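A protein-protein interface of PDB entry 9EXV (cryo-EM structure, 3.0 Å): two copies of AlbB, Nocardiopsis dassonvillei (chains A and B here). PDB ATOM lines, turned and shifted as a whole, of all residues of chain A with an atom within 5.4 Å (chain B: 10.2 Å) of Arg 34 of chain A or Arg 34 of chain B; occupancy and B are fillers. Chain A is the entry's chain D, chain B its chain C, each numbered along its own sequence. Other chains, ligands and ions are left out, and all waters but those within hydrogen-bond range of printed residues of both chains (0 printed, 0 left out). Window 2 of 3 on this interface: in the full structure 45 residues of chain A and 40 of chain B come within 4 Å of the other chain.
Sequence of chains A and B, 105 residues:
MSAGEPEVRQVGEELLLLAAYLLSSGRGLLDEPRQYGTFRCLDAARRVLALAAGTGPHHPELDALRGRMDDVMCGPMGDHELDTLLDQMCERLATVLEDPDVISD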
ATOM      1  N   LEU A  29      16.675 -20.185 -10.161  1.00  0.00           N
ATOM      2  CA  LEU A  29      17.066 -19.039  -9.349  1.00  0.00           C
ATOM      3  C   LEU A  29      15.885 -18.143  -8.997  1.00  0.00           C
ATOM      4  O   LEU A  29      15.989 -17.335  -8.069  1.00  0.00           O
ATOM      5  CB  LEU A  29      18.148 -18.228 -10.066  1.00  0.00           C
ATOM      6  CG  LEU A  29      19.542 -18.862 -10.106  1.00  0.00           C
ATOM      7  CD1 LEU A  29      20.491 -18.045 -10.970  1.00  0.00           C
ATOM      8  CD2 LEU A  29      20.105 -19.026  -8.703  1.00  0.00           C
ATOM      9  N   LEU A  30      14.765 -18.268  -9.712  1.00  0.00           N
ATOM     10  CA  LEU A  30      13.556 -17.523  -9.378  1.00  0.00           C
ATOM     11  C   LEU A  30      12.883 -18.033  -8.111  1.00  0.00           C
ATOM     12  O   LEU A  30      11.894 -17.439  -7.670  1.00  0.00           O
ATOM     13  CB  LEU A  30      12.575 -17.575 -10.548  1.00  0.00           C
ATOM     14  CG  LEU A  30      13.176 -17.224 -11.909  1.00  0.00           C
ATOM     15  CD1 LEU A  30      12.125 -17.282 -12.999  1.00  0.00           C
ATOM     16  CD2 LEU A  30      13.816 -15.853 -11.862  1.00  0.00           C
ATOM     17  N   ASP A  31      13.382 -19.128  -7.537  1.00  0.00           N
ATOM     18  CA  ASP A  31      12.897 -19.664  -6.271  1.00  0.00           C
ATOM     19  C   ASP A  31      13.992 -19.879  -5.239  1.00  0.00           C
ATOM     20  O   ASP A  31      13.677 -19.976  -4.047  1.00  0.00           O
ATOM     21  CB  ASP A  31      12.170 -20.998  -6.496  1.00  0.00           C
ATOM     22  CG  ASP A  31      10.877 -20.839  -7.269  1.00  0.00           C
ATOM     23  OD1 ASP A  31      10.219 -19.788  -7.121  1.00  0.00           O
ATOM     24  OD2 ASP A  31      10.514 -21.767  -8.023  1.00  0.00           O
ATOM     25  N   GLU A  32      15.259 -19.960  -5.648  1.00  0.00           N
ATOM     26  CA  GLU A  32      16.353 -20.190  -4.725  1.00  0.00           C
ATOM     27  C   GLU A  32      16.643 -18.926  -3.920  1.00  0.00           C
ATOM     28  O   GLU A  32      16.231 -17.830  -4.305  1.00  0.00           O
ATOM     29  CB  GLU A  32      17.606 -20.625  -5.486  1.00  0.00           C
ATOM     30  CG  GLU A  32      17.385 -21.698  -6.538  1.00  0.00           C
ATOM     31  CD  GLU A  32      17.195 -23.082  -5.954  1.00  0.00           C
ATOM     32  OE1 GLU A  32      17.212 -23.219  -4.713  1.00  0.00           O
ATOM     33  OE2 GLU A  32      17.033 -24.035  -6.743  1.00  0.00           O
ATOM     34  N   PRO A  33      17.361 -19.048  -2.793  1.00  0.00           N
ATOM     35  CA  PRO A  33      17.697 -17.847  -2.017  1.00  0.00           C
ATOM     36  C   PRO A  33      18.579 -16.884  -2.798  1.00  0.00           C
ATOM     37  O   PRO A  33      18.984 -17.170  -3.928  1.00  0.00           O
ATOM     38  CB  PRO A  33      18.422 -18.411  -0.787  1.00  0.00           C
ATOM     39  CG  PRO A  33      18.902 -19.753  -1.203  1.00  0.00           C
ATOM     40  CD  PRO A  33      17.868 -20.274  -2.150  1.00  0.00           C
ATOM     41  N   ARG A  34      18.875 -15.730  -2.195  1.00  0.00           N
ATOM     42  CA  ARG A  34      19.566 -14.667  -2.917  1.00  0.00           C
ATOM     43  C   ARG A  34      20.978 -15.064  -3.323  1.00  0.00           C
ATOM     44  O   ARG A  34      21.475 -14.606  -4.357  1.00  0.00           O
ATOM     45  CB  ARG A  34      19.609 -13.397  -2.068  1.00  0.00           C
ATOM     46  CG  ARG A  34      18.286 -12.996  -1.426  1.00  0.00           C
ATOM     47  CD  ARG A  34      17.219 -12.676  -2.461  1.00  0.00           C
ATOM     48  NE  ARG A  34      16.524 -13.872  -2.921  1.00  0.00           N
ATOM     49  CZ  ARG A  34      15.543 -14.469  -2.260  1.00  0.00           C
ATOM     50  NH1 ARG A  34      15.120 -14.015  -1.092  1.00  0.00           N
ATOM     51  NH2 ARG A  34      14.973 -15.551  -2.783  1.00  0.00           N
ATOM     52  N   GLN A  35      21.637 -15.907  -2.530  1.00  0.00           N
ATOM     53  CA  GLN A  35      23.071 -16.129  -2.676  1.00  0.00           C
ATOM     54  C   GLN A  35      23.428 -17.166  -3.734  1.00  0.00           C
ATOM     55  O   GLN A  35      24.616 -17.338  -4.026  1.00  0.00           O
ATOM     56  CB  GLN A  35      23.671 -16.547  -1.333  1.00  0.00           C
ATOM     57  CG  GLN A  35      25.157 -16.261  -1.196  1.00  0.00           C
ATOM     58  CD  GLN A  35      25.454 -14.779  -1.088  1.00  0.00           C
ATOM     59  OE1 GLN A  35      26.000 -14.180  -2.003  1.00  0.00           O
ATOM     60  NE2 GLN A  35      25.092 -14.187   0.044  1.00  0.00           N
ATOM     61  N   TYR A  36      22.450 -17.861  -4.311  1.00  0.00           N
ATOM     62  CA  TYR A  36      22.758 -18.896  -5.290  1.00  0.00           C
ATOM     63  C   TYR A  36      23.061 -18.339  -6.674  1.00  0.00           C
ATOM     64  O   TYR A  36      23.517 -19.097  -7.538  1.00  0.00           O
ATOM     65  CB  TYR A  36      21.614 -19.908  -5.372  1.00  0.00           C
ATOM     66  CG  TYR A  36      21.603 -20.900  -4.227  1.00  0.00           C
ATOM     67  CD1 TYR A  36      22.433 -20.728  -3.126  1.00  0.00           C
ATOM     68  CD2 TYR A  36      20.777 -22.015  -4.254  1.00  0.00           C
ATOM     69  CE1 TYR A  36      22.434 -21.629  -2.082  1.00  0.00           C
ATOM     70  CE2 TYR A  36      20.772 -22.925  -3.212  1.00  0.00           C
ATOM     71  CZ  TYR A  36      21.603 -22.726  -2.130  1.00  0.00           C
ATOM     72  OH  TYR A  36      21.608 -23.623  -1.088  1.00  0.00           O
ATOM     73  N   GLY A  37      22.840 -17.043  -6.903  1.00  0.00           N
ATOM     74  CA  GLY A  37      23.209 -16.466  -8.183  1.00  0.00           C
ATOM     75  C   GLY A  37      24.678 -16.667  -8.504  1.00  0.00           C
ATOM     76  O   GLY A  37      25.037 -17.000  -9.636  1.00  0.00           O
ATOM     77  N   SER B  25      30.549 -12.993 -14.073  1.00  0.00           N
ATOM     78  CA  SER B  25      29.126 -12.799 -13.813  1.00  0.00           C
ATOM     79  C   SER B  25      28.769 -13.207 -12.391  1.00  0.00           C
ATOM     80  O   SER B  25      27.987 -12.525 -11.720  1.00  0.00           O
ATOM     81  CB  SER B  25      28.293 -13.586 -14.821  1.00  0.00           C
ATOM     82  OG  SER B  25      28.548 -14.974 -14.718  1.00  0.00           O
ATOM     83  N   GLY B  26      29.330 -14.320 -11.916  1.00  0.00           N
ATOM     84  CA  GLY B  26      29.086 -14.720 -10.540  1.00  0.00           C
ATOM     85  C   GLY B  26      29.563 -13.680  -9.547  1.00  0.00           C
ATOM     86  O   GLY B  26      28.831 -13.284  -8.647  1.00  0.00           O
ATOM     87  N   GLY B  28      30.016 -10.512 -10.045  1.00  0.00           N
ATOM     88  CA  GLY B  28      29.218  -9.305 -10.161  1.00  0.00           C
ATOM     89  C   GLY B  28      27.811  -9.446  -9.619  1.00  0.00           C
ATOM     90  O   GLY B  28      27.226  -8.469  -9.150  1.00  0.00           O
ATOM     91  N   LEU B  29      27.253 -10.659  -9.656  1.00  0.00           N
ATOM     92  CA  LEU B  29      25.864 -10.849  -9.249  1.00  0.00           C
ATOM     93  C   LEU B  29      25.618 -10.438  -7.804  1.00  0.00           C
ATOM     94  O   LEU B  29      24.471 -10.158  -7.440  1.00  0.00           O
ATOM     95  CB  LEU B  29      25.446 -12.303  -9.459  1.00  0.00           C
ATOM     96  CG  LEU B  29      24.895 -12.644 -10.846  1.00  0.00           C
ATOM     97  CD1 LEU B  29      24.584 -14.127 -10.963  1.00  0.00           C
ATOM     98  CD2 LEU B  29      23.657 -11.812 -11.148  1.00  0.00           C
ATOM     99  N   LEU B  30      26.660 -10.402  -6.973  1.00  0.00           N
ATOM    100  CA  LEU B  30      26.497  -9.906  -5.612  1.00  0.00           C
ATOM    101  C   LEU B  30      26.080  -8.443  -5.609  1.00  0.00           C
ATOM    102  O   LEU B  30      25.190  -8.041  -4.849  1.00  0.00           O
ATOM    103  CB  LEU B  30      27.793 -10.106  -4.831  1.00  0.00           C
ATOM    104  CG  LEU B  30      28.207 -11.571  -4.707  1.00  0.00           C
ATOM    105  CD1 LEU B  30      29.712 -11.715  -4.566  1.00  0.00           C
ATOM    106  CD2 LEU B  30      27.495 -12.219  -3.540  1.00  0.00           C
ATOM    107  N   ASP B  31      26.710  -7.629  -6.458  1.00  0.00           N
ATOM    108  CA  ASP B  31      26.335  -6.224  -6.560  1.00  0.00           C
ATOM    109  C   ASP B  31      25.009  -6.059  -7.296  1.00  0.00           C
ATOM    110  O   ASP B  31      24.155  -5.268  -6.880  1.00  0.00           O
ATOM    111  CB  ASP B  31      27.439  -5.440  -7.265  1.00  0.00           C
ATOM    112  CG  ASP B  31      28.813  -5.727  -6.692  1.00  0.00           C
ATOM    113  OD1 ASP B  31      28.906  -6.000  -5.477  1.00  0.00           O
ATOM    114  OD2 ASP B  31      29.799  -5.684  -7.457  1.00  0.00           O
ATOM    115  N   GLU B  32      24.823  -6.796  -8.386  1.00  0.00           N
ATOM    116  CA  GLU B  32      23.606  -6.681  -9.169  1.00  0.00           C
ATOM    117  C   GLU B  32      22.415  -7.236  -8.391  1.00  0.00           C
ATOM    118  O   GLU B  32      22.577  -8.097  -7.523  1.00  0.00           O
ATOM    119  CB  GLU B  32      23.756  -7.422 -10.496  1.00  0.00           C
ATOM    120  CG  GLU B  32      24.334  -6.572 -11.619  1.00  0.00           C
ATOM    121  CD  GLU B  32      25.639  -5.904 -11.252  1.00  0.00           C
ATOM    122  OE1 GLU B  32      26.482  -6.553 -10.610  1.00  0.00           O
ATOM    123  OE2 GLU B  32      25.822  -4.721 -11.605  1.00  0.00           O
ATOM    124  N   PRO B  33      21.205  -6.755  -8.681  1.00  0.00           N
ATOM    125  CA  PRO B  33      20.023  -7.235  -7.955  1.00  0.00           C
ATOM    126  C   PRO B  33      19.790  -8.725  -8.168  1.00  0.00           C
ATOM    127  O   PRO B  33      20.459  -9.395  -8.957  1.00  0.00           O
ATOM    128  CB  PRO B  33      18.877  -6.398  -8.538  1.00  0.00           C
ATOM    129  CG  PRO B  33      19.402  -5.852  -9.828  1.00  0.00           C
ATOM    130  CD  PRO B  33      20.872  -5.680  -9.631  1.00  0.00           C
ATOM    131  N   ARG B  34      18.813  -9.247  -7.423  1.00  0.00           N
ATOM    132  CA  ARG B  34      18.503 -10.673  -7.483  1.00  0.00           C
ATOM    133  C   ARG B  34      18.019 -11.085  -8.864  1.00  0.00           C
ATOM    134  O   ARG B  34      18.382 -12.155  -9.368  1.00  0.00           O
ATOM    135  CB  ARG B  34      17.453 -11.020  -6.428  1.00  0.00           C
ATOM    136  CG  ARG B  34      16.967 -12.464  -6.452  1.00  0.00           C
ATOM    137  CD  ARG B  34      15.557 -12.557  -5.891  1.00  0.00           C
ATOM    138  NE  ARG B  34      15.127 -13.934  -5.675  1.00  0.00           N
ATOM    139  CZ  ARG B  34      14.230 -14.578  -6.413  1.00  0.00           C
ATOM    140  NH1 ARG B  34      13.652 -14.008  -7.457  1.00  0.00           N
ATOM    141  NH2 ARG B  34      13.899 -15.823  -6.086  1.00  0.00           N
ATOM    142  N   GLN B  35      17.187 -10.251  -9.493  1.00  0.00           N
ATOM    143  CA  GLN B  35      16.591 -10.617 -10.771  1.00  0.00           C
ATOM    144  C   GLN B  35      17.635 -10.828 -11.860  1.00  0.00           C
ATOM    145  O   GLN B  35      17.343 -11.485 -12.863  1.00  0.00           O
ATOM    146  CB  GLN B  35      15.587  -9.548 -11.196  1.00  0.00           C
ATOM    147  CG  GLN B  35      14.401  -9.420 -10.253  1.00  0.00           C
ATOM    148  CD  GLN B  35      13.495 -10.635 -10.295  1.00  0.00           C
ATOM    149  OE1 GLN B  35      13.244 -11.198 -11.360  1.00  0.00           O
ATOM    150  NE2 GLN B  35      13.004 -11.050  -9.132  1.00  0.00           N
ATOM    151  N   TYR B  36      18.846 -10.298 -11.678  1.00  0.00           N
ATOM    152  CA  TYR B  36      19.887 -10.452 -12.684  1.00  0.00           C
ATOM    153  C   TYR B  36      20.493 -11.849 -12.704  1.00  0.00           C
ATOM    154  O   TYR B  36      21.170 -12.196 -13.674  1.00  0.00           O
ATOM    155  CB  TYR B  36      20.993  -9.421 -12.467  1.00  0.00           C
ATOM    156  CG  TYR B  36      20.702  -8.071 -13.080  1.00  0.00           C
ATOM    157  CD1 TYR B  36      19.399  -7.652 -13.306  1.00  0.00           C
ATOM    158  CD2 TYR B  36      21.732  -7.224 -13.455  1.00  0.00           C
ATOM    159  CE1 TYR B  36      19.131  -6.422 -13.871  1.00  0.00           C
ATOM    160  CE2 TYR B  36      21.479  -5.992 -14.019  1.00  0.00           C
ATOM    161  CZ  TYR B  36      20.176  -5.595 -14.227  1.00  0.00           C
ATOM    162  OH  TYR B  36      19.916  -4.370 -14.793  1.00  0.00           O
ATOM    163  N   GLY B  37      20.283 -12.654 -11.660  1.00  0.00           N
ATOM    164  CA  GLY B  37      20.835 -14.000 -11.671  1.00  0.00           C
ATOM    165  C   GLY B  37      20.298 -14.835 -12.817  1.00  0.00           C
ATOM    166  O   GLY B  37      21.058 -15.462 -13.557  1.00  0.00           O
ATOM    167  N   THR B  38      18.976 -14.828 -12.993  1.00  0.00           N
ATOM    168  CA  THR B  38      18.370 -15.592 -14.075  1.00  0.00           C
ATOM    169  C   THR B  38      18.802 -15.061 -15.433  1.00  0.00           C
ATOM    170  O   THR B  38      19.020 -15.837 -16.372  1.00  0.00           O
ATOM    171  CB  THR B  38      16.850 -15.562 -13.956  1.00  0.00           C
ATOM    172  OG1 THR B  38      16.468 -16.195 -12.734  1.00  0.00           O
ATOM    173  CG2 THR B  38      16.210 -16.283 -15.129  1.00  0.00           C
ATOM    174  N   PHE B  39      18.915 -13.739 -15.564  1.00  0.00           N
ATOM    175  CA  PHE B  39      19.324 -13.166 -16.841  1.00  0.00           C
ATOM    176  C   PHE B  39      20.765 -13.520 -17.174  1.00  0.00           C
ATOM    177  O   PHE B  39      21.092 -13.766 -18.340  1.00  0.00           O
ATOM    178  CB  PHE B  39      19.135 -11.656 -16.827  1.00  0.00           C
ATOM    179  CG  PHE B  39      17.706 -11.240 -16.882  1.00  0.00           C
ATOM    180  CD1 PHE B  39      16.963 -11.452 -18.027  1.00  0.00           C
ATOM    181  CD2 PHE B  39      17.098 -10.655 -15.789  1.00  0.00           C
ATOM    182  CE1 PHE B  39      15.646 -11.073 -18.088  1.00  0.00           C
ATOM    183  CE2 PHE B  39      15.776 -10.272 -15.841  1.00  0.00           C
ATOM    184  CZ  PHE B  39      15.047 -10.483 -16.995  1.00  0.00           C
ATOM    185  N   ARG B  40      21.642 -13.529 -16.174  1.00  0.00           N
ATOM    186  CA  ARG B  40      23.020 -13.931 -16.428  1.00  0.00           C
ATOM    187  C   ARG B  40      23.095 -15.407 -16.797  1.00  0.00           C
ATOM    188  O   ARG B  40      23.862 -15.793 -17.686  1.00  0.00           O
ATOM    189  CB  ARG B  40      23.881 -13.603 -15.212  1.00  0.00           C
ATOM    190  CG  ARG B  40      23.960 -12.108 -14.913  1.00  0.00           C
ATOM    191  CD  ARG B  40      24.876 -11.379 -15.882  1.00  0.00           C
ATOM    192  NE  ARG B  40      25.731 -10.423 -15.188  1.00  0.00           N
ATOM    193  CZ  ARG B  40      25.373  -9.188 -14.862  1.00  0.00           C
ATOM    194  NH1 ARG B  40      24.176  -8.714 -15.163  1.00  0.00           N
ATOM    195  NH2 ARG B  40      26.237  -8.412 -14.214  1.00  0.00           N
ATOM    196  N   CYS B  41      22.279 -16.242 -16.152  1.00  0.00           N
ATOM    197  CA  CYS B  41      22.202 -17.646 -16.540  1.00  0.00           C
ATOM    198  C   CYS B  41      21.714 -17.800 -17.977  1.00  0.00           C
ATOM    199  O   CYS B  41      22.265 -18.598 -18.746  1.00  0.00           O
ATOM    200  CB  CYS B  41      21.292 -18.409 -15.578  1.00  0.00           C
ATOM    201  N   LEU B  82      10.134 -13.665 -16.562  1.00  0.00           N
ATOM    202  CA  LEU B  82      11.136 -14.722 -16.621  1.00  0.00           C
ATOM    203  C   LEU B  82      10.627 -16.089 -16.200  1.00  0.00           C
ATOM    204  O   LEU B  82      11.139 -17.091 -16.702  1.00  0.00           O
ATOM    205  CB  LEU B  82      12.348 -14.363 -15.768  1.00  0.00           C
ATOM    206  CG  LEU B  82      13.332 -13.348 -16.339  1.00  0.00           C
ATOM    207  CD1 LEU B  82      14.476 -13.220 -15.354  1.00  0.00           C
ATOM    208  CD2 LEU B  82      13.831 -13.708 -17.744  1.00  0.00           C
ATOM    209  N   ASP B  83       9.669 -16.191 -15.282  1.00  0.00           N
ATOM    210  CA  ASP B  83       9.222 -17.531 -14.912  1.00  0.00           C
ATOM    211  C   ASP B  83       8.684 -18.275 -16.130  1.00  0.00           C
ATOM    212  O   ASP B  83       9.181 -19.349 -16.485  1.00  0.00           O
ATOM    213  CB  ASP B  83       8.201 -17.478 -13.766  1.00  0.00           C
ATOM    214  CG  ASP B  83       7.031 -16.545 -14.038  1.00  0.00           C
ATOM    215  OD1 ASP B  83       7.056 -15.797 -15.018  1.00  0.00           O
ATOM    216  OD2 ASP B  83       6.069 -16.569 -13.242  1.00  0.00           O
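The side-chain amide nitrogen (NE2) of Gln 35 of chain B sits close to the guanidinium group (NH1) of Arg 34 of chain B (3.5 Å).
The backbone carbonyl oxygen of Glu 32 of chain A sits at hydrogen-bond distance from the guanidinium group of Arg 34 of chain A, at 3.0 Å.
Of the printed residues of chain B, Arg 34 of chain A touches Arg 34.
Of chain A, only Leu 29 (3.3 Å), Leu 30 (3.0 Å), Asp 31 (3.6 Å), Glu 32 (3.6 Å) and Arg 34 (3.1 Å) come within 4 Å of Arg 34 of chain B.
No residue of chain B comes within 4 Å of Pro 33 of chain A.
Of chain B, only Leu 30 comes within 4 Å of Gln 35 of chain A.
Of the printed residues of chain A, Leu 29 of chain B touches Gly 37 (3.2 Å).
Of the printed residues of chain A, Leu 30 of chain B touches Gln 35 (2.9 Å).
Of the printed residues of chain A, Gly 37 of chain B touches Leu 29 (3.7 Å).
Printed residues of chain A within 4 Å of Thr 38 of chain B: Leu 29 and Leu 30.
Printed residues of chain A within 4 Å of Asp 83 of chain B: Leu 30.
Gly 26 of chain B touches none of the printed residues of chain A.
The nearest residue of chain A that does not touch Arg 34 of chain B is Pro 33 of chain A (5.3 Å).
Among the printed residues, pairs that only touch across the chains: Leu 29 of chain A with Gly 37 of chain B, Leu 29 of chain A with Thr 38 of chain B, Leu 30 of chain A with Thr 38 of chain B, Leu 30 of chain A with Leu 82 of chain B, Leu 30 of chain A with Asp 83 of chain B, Asp 31 of chain A with Arg 34 of chain B, Glu 32 of chain A with Arg 34 of chain B, Gln 35 of chain A with Leu 30 of chain B and Gly 37 of chain A with Leu 29 of chain B.
Leu 30 of chain A touches Arg 34 of chain B, but with the chains exchanged Arg 34 of chain A does not touch Leu 30 of chain B (6.5 Å).
Asp 31 of chain A touches Arg 34 of chain B, but with the chains exchanged Arg 34 of chain A does not touch Asp 31 of chain B (9.0 Å).
Arg 34 of chain A touches its own counterpart, Arg 34 of chain B.
Gln 35 of chain A touches Leu 30 of chain B, but with the chains exchanged Leu 30 of chain A does not touch Gln 35 of chain B (4.7 Å).
Of the 12 pairs that touch across the chains among the printed residues, 3 have their exchanged pair printed and touching as well.
The guanidinium group of Arg 34 of chain B is in hydrogen-bond range of the backbone carbonyl oxygen of Leu 29 of chain A.
The guanidinium group (NH2) of Arg 34 of chain B lies within hydrogen-bond range of the backbone carbonyl oxygen (O) of Leu 30 of chain A.
The guanidinium group of Arg 34 of chain A lies close to the guanidinium group of Arg 34 of chain B (3.1 Å).
Hydrophobic or aromatic side chains of chain B within 4 Å of the printed part of chain A: Leu 29 and Leu 30.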
